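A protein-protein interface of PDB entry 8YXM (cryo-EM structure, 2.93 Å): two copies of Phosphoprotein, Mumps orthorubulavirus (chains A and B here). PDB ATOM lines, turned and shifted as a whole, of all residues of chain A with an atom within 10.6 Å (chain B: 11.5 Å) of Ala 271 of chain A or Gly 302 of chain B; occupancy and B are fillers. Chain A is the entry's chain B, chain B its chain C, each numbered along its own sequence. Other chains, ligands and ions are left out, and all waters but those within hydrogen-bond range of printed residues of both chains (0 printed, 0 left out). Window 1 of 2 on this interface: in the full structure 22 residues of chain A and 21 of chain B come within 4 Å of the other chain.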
ATOM      1  N   LEU A 263       3.433  -9.990  15.775  1.00  0.00           N
ATOM      2  CA  LEU A 263       3.661  -8.605  16.169  1.00  0.00           C
ATOM      3  C   LEU A 263       3.666  -7.684  14.957  1.00  0.00           C
ATOM      4  O   LEU A 263       3.146  -6.565  15.018  1.00  0.00           O
ATOM      5  CB  LEU A 263       4.977  -8.494  16.938  1.00  0.00           C
ATOM      6  CG  LEU A 263       5.551  -7.090  17.111  1.00  0.00           C
ATOM      7  CD1 LEU A 263       4.687  -6.273  18.058  1.00  0.00           C
ATOM      8  CD2 LEU A 263       6.986  -7.158  17.606  1.00  0.00           C
ATOM      9  N   ALA A 264       4.251  -8.137  13.844  1.00  0.00           N
ATOM     10  CA  ALA A 264       4.215  -7.346  12.620  1.00  0.00           C
ATOM     11  C   ALA A 264       2.790  -7.186  12.110  1.00  0.00           C
ATOM     12  O   ALA A 264       2.415  -6.114  11.618  1.00  0.00           O
ATOM     13  CB  ALA A 264       5.097  -7.990  11.553  1.00  0.00           C
ATOM     14  N   THR A 265       1.982  -8.245  12.207  1.00  0.00           N
ATOM     15  CA  THR A 265       0.580  -8.138  11.815  1.00  0.00           C
ATOM     16  C   THR A 265      -0.142  -7.096  12.661  1.00  0.00           C
ATOM     17  O   THR A 265      -0.889  -6.261  12.136  1.00  0.00           O
ATOM     18  CB  THR A 265      -0.107  -9.498  11.939  1.00  0.00           C
ATOM     19  OG1 THR A 265       0.315 -10.350  10.868  1.00  0.00           O
ATOM     20  CG2 THR A 265      -1.617  -9.343  11.883  1.00  0.00           C
ATOM     21  N   ILE A 266       0.085  -7.123  13.976  1.00  0.00           N
ATOM     22  CA  ILE A 266      -0.546  -6.146  14.862  1.00  0.00           C
ATOM     23  C   ILE A 266      -0.094  -4.734  14.510  1.00  0.00           C
ATOM     24  O   ILE A 266      -0.901  -3.795  14.474  1.00  0.00           O
ATOM     25  CB  ILE A 266      -0.242  -6.485  16.333  1.00  0.00           C
ATOM     26  CG1 ILE A 266      -0.854  -7.835  16.711  1.00  0.00           C
ATOM     27  CG2 ILE A 266      -0.745  -5.383  17.253  1.00  0.00           C
ATOM     28  CD1 ILE A 266      -2.230  -7.739  17.323  1.00  0.00           C
ATOM     29  N   GLU A 267       1.203  -4.563  14.248  1.00  0.00           N
ATOM     30  CA  GLU A 267       1.734  -3.250  13.890  1.00  0.00           C
ATOM     31  C   GLU A 267       1.099  -2.719  12.612  1.00  0.00           C
ATOM     32  O   GLU A 267       0.688  -1.554  12.553  1.00  0.00           O
ATOM     33  CB  GLU A 267       3.251  -3.336  13.731  1.00  0.00           C
ATOM     34  CG  GLU A 267       4.000  -2.072  14.090  1.00  0.00           C
ATOM     35  CD  GLU A 267       5.216  -1.858  13.212  1.00  0.00           C
ATOM     36  OE1 GLU A 267       5.942  -0.866  13.425  1.00  0.00           O
ATOM     37  OE2 GLU A 267       5.443  -2.687  12.304  1.00  0.00           O
ATOM     38  N   GLY A 268       1.012  -3.558  11.578  1.00  0.00           N
ATOM     39  CA  GLY A 268       0.406  -3.116  10.331  1.00  0.00           C
ATOM     40  C   GLY A 268      -1.065  -2.792  10.488  1.00  0.00           C
ATOM     41  O   GLY A 268      -1.570  -1.821   9.915  1.00  0.00           O
ATOM     42  N   MET A 269      -1.768  -3.593  11.281  1.00  0.00           N
ATOM     43  CA  MET A 269      -3.185  -3.344  11.527  1.00  0.00           C
ATOM     44  C   MET A 269      -3.408  -2.024  12.250  1.00  0.00           C
ATOM     45  O   MET A 269      -4.337  -1.288  11.933  1.00  0.00           O
ATOM     46  CB  MET A 269      -3.810  -4.475  12.342  1.00  0.00           C
ATOM     47  CG  MET A 269      -4.095  -5.738  11.552  1.00  0.00           C
ATOM     48  SD  MET A 269      -4.830  -7.029  12.572  1.00  0.00           S
ATOM     49  CE  MET A 269      -5.222  -8.258  11.330  1.00  0.00           C
ATOM     50  N   MET A 270      -2.560  -1.724  13.227  1.00  0.00           N
ATOM     51  CA  MET A 270      -2.699  -0.457  13.937  1.00  0.00           C
ATOM     52  C   MET A 270      -2.299   0.722  13.058  1.00  0.00           C
ATOM     53  O   MET A 270      -2.885   1.807  13.162  1.00  0.00           O
ATOM     54  CB  MET A 270      -1.884  -0.476  15.226  1.00  0.00           C
ATOM     55  CG  MET A 270      -2.598   0.228  16.356  1.00  0.00           C
ATOM     56  SD  MET A 270      -3.886  -0.806  17.067  1.00  0.00           S
ATOM     57  CE  MET A 270      -5.121   0.432  17.444  1.00  0.00           C
ATOM     58  N   ALA A 271      -1.306   0.535  12.185  1.00  0.00           N
ATOM     59  CA  ALA A 271      -0.955   1.594  11.245  1.00  0.00           C
ATOM     60  C   ALA A 271      -2.116   1.899  10.310  1.00  0.00           C
ATOM     61  O   ALA A 271      -2.419   3.070  10.043  1.00  0.00           O
ATOM     62  CB  ALA A 271       0.288   1.203  10.449  1.00  0.00           C
ATOM     63  N   THR A 272      -2.771   0.856   9.815  1.00  0.00           N
ATOM     64  CA  THR A 272      -3.900   1.047   8.918  1.00  0.00           C
ATOM     65  C   THR A 272      -5.004   1.790   9.636  1.00  0.00           C
ATOM     66  O   THR A 272      -5.606   2.705   9.089  1.00  0.00           O
ATOM     67  CB  THR A 272      -4.449  -0.289   8.409  1.00  0.00           C
ATOM     68  OG1 THR A 272      -3.391  -1.040   7.802  1.00  0.00           O
ATOM     69  CG2 THR A 272      -5.548  -0.052   7.389  1.00  0.00           C
ATOM     70  N   VAL A 273      -5.274   1.400  10.873  1.00  0.00           N
ATOM     71  CA  VAL A 273      -6.287   2.088  11.649  1.00  0.00           C
ATOM     72  C   VAL A 273      -5.927   3.564  11.763  1.00  0.00           C
ATOM     73  O   VAL A 273      -6.743   4.423  11.441  1.00  0.00           O
ATOM     74  CB  VAL A 273      -6.452   1.472  13.047  1.00  0.00           C
ATOM     75  CG1 VAL A 273      -7.282   2.383  13.937  1.00  0.00           C
ATOM     76  CG2 VAL A 273      -7.072   0.088  12.947  1.00  0.00           C
ATOM     77  N   LYS A 274      -4.714   3.872  12.215  1.00  0.00           N
ATOM     78  CA  LYS A 274      -4.373   5.281  12.398  1.00  0.00           C
ATOM     79  C   LYS A 274      -4.523   6.065  11.099  1.00  0.00           C
ATOM     80  O   LYS A 274      -5.057   7.180  11.103  1.00  0.00           O
ATOM     81  CB  LYS A 274      -2.956   5.431  12.945  1.00  0.00           C
ATOM     82  CG  LYS A 274      -2.506   6.884  13.006  1.00  0.00           C
ATOM     83  CD  LYS A 274      -1.139   7.043  13.645  1.00  0.00           C
ATOM     84  CE  LYS A 274      -0.503   8.359  13.232  1.00  0.00           C
ATOM     85  NZ  LYS A 274      -0.699   9.413  14.263  1.00  0.00           N
ATOM     86  N   ILE A 275      -4.116   5.483   9.975  1.00  0.00           N
ATOM     87  CA  ILE A 275      -4.221   6.173   8.689  1.00  0.00           C
ATOM     88  C   ILE A 275      -5.645   6.205   8.142  1.00  0.00           C
ATOM     89  O   ILE A 275      -5.871   6.699   7.040  1.00  0.00           O
ATOM     90  CB  ILE A 275      -3.295   5.552   7.616  1.00  0.00           C
ATOM     91  CG1 ILE A 275      -3.718   4.123   7.275  1.00  0.00           C
ATOM     92  CG2 ILE A 275      -1.849   5.579   8.081  1.00  0.00           C
ATOM     93  CD1 ILE A 275      -4.618   4.008   6.063  1.00  0.00           C
ATOM     94  N   MET A 276      -6.604   5.682   8.898  1.00  0.00           N
ATOM     95  CA  MET A 276      -7.991   5.645   8.430  1.00  0.00           C
ATOM     96  C   MET A 276      -8.825   6.775   9.013  1.00  0.00           C
ATOM     97  O   MET A 276     -10.034   6.815   8.816  1.00  0.00           O
ATOM     98  CB  MET A 276      -8.650   4.306   8.760  1.00  0.00           C
ATOM     99  CG  MET A 276      -8.400   3.205   7.743  1.00  0.00           C
ATOM    100  SD  MET A 276      -9.327   1.709   8.136  1.00  0.00           S
ATOM    101  CE  MET A 276      -8.973   0.691   6.707  1.00  0.00           C
ATOM    102  N   ASP A 277      -8.185   7.690   9.731  1.00  0.00           N
ATOM    103  CA  ASP A 277      -8.897   8.825  10.302  1.00  0.00           C
ATOM    104  C   ASP A 277      -8.948   9.967   9.302  1.00  0.00           C
ATOM    105  O   ASP A 277      -7.917  10.546   8.967  1.00  0.00           O
ATOM    106  CB  ASP A 277      -8.224   9.285  11.592  1.00  0.00           C
ATOM    107  CG  ASP A 277      -8.922  10.469  12.227  1.00  0.00           C
ATOM    108  OD1 ASP A 277     -10.082  10.753  11.862  1.00  0.00           O
ATOM    109  OD2 ASP A 277      -8.312  11.117  13.104  1.00  0.00           O
ATOM    110  N   ASN A 280      -7.028  13.605   9.812  1.00  0.00           N
ATOM    111  CA  ASN A 280      -5.668  13.954   9.425  1.00  0.00           C
ATOM    112  C   ASN A 280      -5.296  13.327   8.095  1.00  0.00           C
ATOM    113  O   ASN A 280      -5.049  12.126   8.026  1.00  0.00           O
ATOM    114  CB  ASN A 280      -4.677  13.491  10.489  1.00  0.00           C
ATOM    115  CG  ASN A 280      -4.998  14.035  11.866  1.00  0.00           C
ATOM    116  OD1 ASN A 280      -6.092  14.539  12.112  1.00  0.00           O
ATOM    117  ND2 ASN A 280      -4.040  13.926  12.778  1.00  0.00           N
ATOM    118  N   THR A 282      -3.280  11.856   5.074  1.00  0.00           N
ATOM    119  CA  THR A 282      -2.018  11.134   5.082  1.00  0.00           C
ATOM    120  C   THR A 282      -1.438  11.069   3.677  1.00  0.00           C
ATOM    121  O   THR A 282      -2.169  11.112   2.683  1.00  0.00           O
ATOM    122  CB  THR A 282      -2.195   9.715   5.630  1.00  0.00           C
ATOM    123  OG1 THR A 282      -3.461   9.193   5.202  1.00  0.00           O
ATOM    124  CG2 THR A 282      -2.147   9.724   7.149  1.00  0.00           C
ATOM    125  N   GLY A 283      -0.115  10.966   3.608  1.00  0.00           N
ATOM    126  CA  GLY A 283       0.569  10.859   2.336  1.00  0.00           C
ATOM    127  C   GLY A 283       1.466   9.643   2.243  1.00  0.00           C
ATOM    128  O   GLY A 283       2.217   9.344   3.175  1.00  0.00           O
ATOM    129  N   VAL A 284       1.390   8.931   1.129  1.00  0.00           N
ATOM    130  CA  VAL A 284       2.247   7.757   0.926  1.00  0.00           C
ATOM    131  C   VAL A 284       3.681   8.220   0.700  1.00  0.00           C
ATOM    132  O   VAL A 284       3.906   9.161  -0.082  1.00  0.00           O
ATOM    133  CB  VAL A 284       1.744   6.933  -0.259  1.00  0.00           C
ATOM    134  CG1 VAL A 284       2.275   5.520  -0.182  1.00  0.00           C
ATOM    135  CG2 VAL A 284       0.233   6.932  -0.291  1.00  0.00           C
ATOM    136  N   PRO A 285       4.671   7.625   1.361  1.00  0.00           N
ATOM    137  CA  PRO A 285       6.063   8.001   1.088  1.00  0.00           C
ATOM    138  C   PRO A 285       6.421   7.752  -0.369  1.00  0.00           C
ATOM    139  O   PRO A 285       6.052   6.729  -0.950  1.00  0.00           O
ATOM    140  CB  PRO A 285       6.866   7.099   2.032  1.00  0.00           C
ATOM    141  CG  PRO A 285       5.908   6.738   3.114  1.00  0.00           C
ATOM    142  CD  PRO A 285       4.568   6.645   2.454  1.00  0.00           C
ATOM    143  N   MET B 270      -8.163  -7.302  17.417  1.00  0.00           N
ATOM    144  CA  MET B 270      -7.823  -6.226  16.496  1.00  0.00           C
ATOM    145  C   MET B 270      -8.321  -6.541  15.099  1.00  0.00           C
ATOM    146  O   MET B 270      -8.700  -5.642  14.353  1.00  0.00           O
ATOM    147  CB  MET B 270      -6.314  -6.000  16.473  1.00  0.00           C
ATOM    148  CG  MET B 270      -5.875  -4.813  15.636  1.00  0.00           C
ATOM    149  SD  MET B 270      -4.132  -4.447  15.894  1.00  0.00           S
ATOM    150  CE  MET B 270      -4.100  -4.283  17.677  1.00  0.00           C
ATOM    151  N   ALA B 271      -8.334  -7.818  14.748  1.00  0.00           N
ATOM    152  CA  ALA B 271      -8.794  -8.216  13.429  1.00  0.00           C
ATOM    153  C   ALA B 271     -10.305  -8.087  13.314  1.00  0.00           C
ATOM    154  O   ALA B 271     -10.841  -8.040  12.213  1.00  0.00           O
ATOM    155  CB  ALA B 271      -8.361  -9.640  13.134  1.00  0.00           C
ATOM    156  N   VAL B 273     -12.162  -5.556  14.829  1.00  0.00           N
ATOM    157  CA  VAL B 273     -12.596  -4.235  15.263  1.00  0.00           C
ATOM    158  C   VAL B 273     -13.562  -3.616  14.265  1.00  0.00           C
ATOM    159  O   VAL B 273     -13.732  -4.127  13.160  1.00  0.00           O
ATOM    160  CB  VAL B 273     -11.404  -3.287  15.463  1.00  0.00           C
ATOM    161  CG1 VAL B 273     -10.519  -3.778  16.596  1.00  0.00           C
ATOM    162  CG2 VAL B 273     -10.611  -3.152  14.174  1.00  0.00           C
ATOM    163  N   ILE B 275     -14.626  -0.105  12.187  1.00  0.00           N
ATOM    164  CA  ILE B 275     -14.277   1.250  11.794  1.00  0.00           C
ATOM    165  C   ILE B 275     -15.560   2.026  11.602  1.00  0.00           C
ATOM    166  O   ILE B 275     -16.315   1.749  10.675  1.00  0.00           O
ATOM    167  CB  ILE B 275     -13.458   1.269  10.494  1.00  0.00           C
ATOM    168  CG1 ILE B 275     -12.260   0.325  10.610  1.00  0.00           C
ATOM    169  CG2 ILE B 275     -12.997   2.681  10.178  1.00  0.00           C
ATOM    170  CD1 ILE B 275     -11.340   0.652  11.764  1.00  0.00           C
ATOM    171  N   VAL B 297      -0.008  14.454   5.737  1.00  0.00           N
ATOM    172  CA  VAL B 297       1.159  14.051   6.502  1.00  0.00           C
ATOM    173  C   VAL B 297       1.705  12.788   5.874  1.00  0.00           C
ATOM    174  O   VAL B 297       0.971  11.826   5.700  1.00  0.00           O
ATOM    175  CB  VAL B 297       0.807  13.783   7.969  1.00  0.00           C
ATOM    176  CG1 VAL B 297       2.031  13.984   8.846  1.00  0.00           C
ATOM    177  CG2 VAL B 297      -0.333  14.685   8.420  1.00  0.00           C
ATOM    178  N   THR B 298       2.996  12.759   5.571  1.00  0.00           N
ATOM    179  CA  THR B 298       3.556  11.602   4.878  1.00  0.00           C
ATOM    180  C   THR B 298       4.019  10.543   5.859  1.00  0.00           C
ATOM    181  O   THR B 298       5.216  10.333   6.037  1.00  0.00           O
ATOM    182  CB  THR B 298       4.723  11.998   3.957  1.00  0.00           C
ATOM    183  OG1 THR B 298       4.424  13.243   3.315  1.00  0.00           O
ATOM    184  CG2 THR B 298       4.947  10.934   2.897  1.00  0.00           C
ATOM    185  N   ILE B 299       3.072   9.879   6.505  1.00  0.00           N
ATOM    186  CA  ILE B 299       3.413   8.825   7.451  1.00  0.00           C
ATOM    187  C   ILE B 299       3.327   7.488   6.732  1.00  0.00           C
ATOM    188  O   ILE B 299       2.495   7.300   5.836  1.00  0.00           O
ATOM    189  CB  ILE B 299       2.509   8.854   8.701  1.00  0.00           C
ATOM    190  CG1 ILE B 299       1.174   8.156   8.444  1.00  0.00           C
ATOM    191  CG2 ILE B 299       2.276  10.281   9.154  1.00  0.00           C
ATOM    192  CD1 ILE B 299       0.581   7.531   9.684  1.00  0.00           C
ATOM    193  N   VAL B 300       4.216   6.573   7.098  1.00  0.00           N
ATOM    194  CA  VAL B 300       4.311   5.272   6.451  1.00  0.00           C
ATOM    195  C   VAL B 300       3.413   4.284   7.182  1.00  0.00           C
ATOM    196  O   VAL B 300       3.468   4.168   8.413  1.00  0.00           O
ATOM    197  CB  VAL B 300       5.769   4.784   6.415  1.00  0.00           C
ATOM    198  CG1 VAL B 300       6.431   4.972   7.773  1.00  0.00           C
ATOM    199  CG2 VAL B 300       5.836   3.331   5.980  1.00  0.00           C
ATOM    200  N   SER B 301       2.571   3.582   6.429  1.00  0.00           N
ATOM    201  CA  SER B 301       1.690   2.557   6.970  1.00  0.00           C
ATOM    202  C   SER B 301       2.194   1.191   6.530  1.00  0.00           C
ATOM    203  O   SER B 301       2.407   0.959   5.335  1.00  0.00           O
ATOM    204  CB  SER B 301       0.248   2.761   6.504  1.00  0.00           C
ATOM    205  OG  SER B 301       0.135   2.579   5.103  1.00  0.00           O
ATOM    206  N   GLY B 302       2.372   0.291   7.490  1.00  0.00           N
ATOM    207  CA  GLY B 302       2.909  -1.015   7.205  1.00  0.00           C
ATOM    208  C   GLY B 302       4.339  -0.943   6.711  1.00  0.00           C
ATOM    209  O   GLY B 302       5.221  -0.381   7.369  1.00  0.00           O
ATOM    210  N   PRO B 303       4.595  -1.514   5.538  1.00  0.00           N
ATOM    211  CA  PRO B 303       5.956  -1.523   4.999  1.00  0.00           C
ATOM    212  C   PRO B 303       6.399  -0.152   4.515  1.00  0.00           C
ATOM    213  O   PRO B 303       5.595   0.684   4.098  1.00  0.00           O
ATOM    214  CB  PRO B 303       5.865  -2.513   3.833  1.00  0.00           C
ATOM    215  CG  PRO B 303       4.446  -2.453   3.403  1.00  0.00           C
ATOM    216  CD  PRO B 303       3.614  -2.081   4.598  1.00  0.00           C
ATOM    217  N   GLY B 304       7.709   0.065   4.572  1.00  0.00           N
ATOM    218  CA  GLY B 304       8.296   1.325   4.159  1.00  0.00           C
ATOM    219  C   GLY B 304       9.428   1.778   5.060  1.00  0.00           C
ATOM    220  O   GLY B 304      10.549   1.274   4.969  1.00  0.00           O
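The backbone carbonyl oxygen of Gly 283 of chain A is in hydrogen-bond range of the backbone NH of Ile 299 of chain B, at 3.5 Å. The backbone NH of Gly 283 of chain A is in hydrogen-bond range of the backbone carbonyl oxygen of Val 297 of chain B (2.5 Å). SD of Met 270 of chain B lies close to O of Ile 266 of chain A (3.6 Å).
Among the printed residues, pairs that only touch across the chains: Gly 283 of chain A with Thr 298 of chain B (3.1 Å), Thr 282 of chain A with Val 297 of chain B (3.1 Å), Ile 275 of chain A with Ile 299 of chain B (3.5 Å), Met 270 of chain A with Met 270 of chain B (3.5 Å), Met 269 of chain A with Met 270 of chain B (3.6 Å), Val 284 of chain A with Thr 298 of chain B (3.6 Å), Pro 285 of chain A with Thr 298 of chain B (3.6 Å), Ala 271 of chain A with Gly 302 of chain B (3.7 Å), Lys 274 of chain A with Ile 299 of chain B (3.8 Å), Pro 285 of chain A with Val 300 of chain B (3.8 Å), Ile 275 of chain A with Ser 301 of chain B (3.9 Å), Met 269 of chain A with Ala 271 of chain B (3.9 Å), Thr 282 of chain A with Ile 299 of chain B (3.9 Å) and Ala 271 of chain A with Ser 301 of chain B (3.99 Å).
Printed residues of chain B within 4 Å of Ala 271 of chain A: Ser 301 (3.99 Å) and Gly 302 (3.7 Å). Of chain A, only Ala 271 comes within 4 Å of Gly 302 of chain B. No residue of chain B comes within 4 Å of Glu 267 of chain A. Printed residues of chain B within 4 Å of Met 270 of chain A: Met 270 (3.5 Å). No residue of chain B comes within 4 Å of Thr 272 of chain A. No residue of chain B comes within 4 Å of Val 273 of chain A. Of chain B, only Ile 299 (3.5 Å) and Ser 301 (3.9 Å) come within 4 Å of Ile 275 of chain A. No residue of chain A comes within 4 Å of Pro 303 of chain B. No residue of chain A comes within 4 Å of Gly 304 of chain B. Of the printed residues of chain B, Ile 266 of chain A touches Met 270 (3.6 Å). Of the printed residues of chain B, Thr 282 of chain A touches Val 297 (3.1 Å) and Ile 299 (3.9 Å). Printed residues of chain A within 4 Å of Ser 301 of chain B: Ala 271 (3.99 Å) and Ile 275 (3.9 Å). Asn 280 of chain A touches none of the printed residues of chain B. The nearest printed residue of chain B that does not touch Ala 271 of chain A is Val 300 of chain B (4.8 Å). The nearest residue of chain A that does not touch Gly 302 of chain B is Gly 268 of chain A (4.5 Å). The nearest printed residue of chain A that does not touch Thr 298 of chain B is Thr 282 of chain A (5.1 Å).
Hydrophobic or aromatic side chains of chain A that line the printed part of chain B: Ile 266, Met 269, Met 270, Ala 271, Ile 275 and Pro 285. Hydrophobic or aromatic side chains of chain B that line the printed part of chain A: Met 270, Ala 271, Ile 299 and Val 300. Among the printed residues, no Asp or Glu carboxylate lies within 4 Å of a Lys or Arg side-chain nitrogen of the other chain.
Met 270 of chain B touches its own counterpart, Met 270 of chain A. Positions printed for both chains: 270, 271, 273 and 275. Of the 17 pairs that touch across the chains among the printed residues, 1 has its exchanged pair printed and touching as well.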
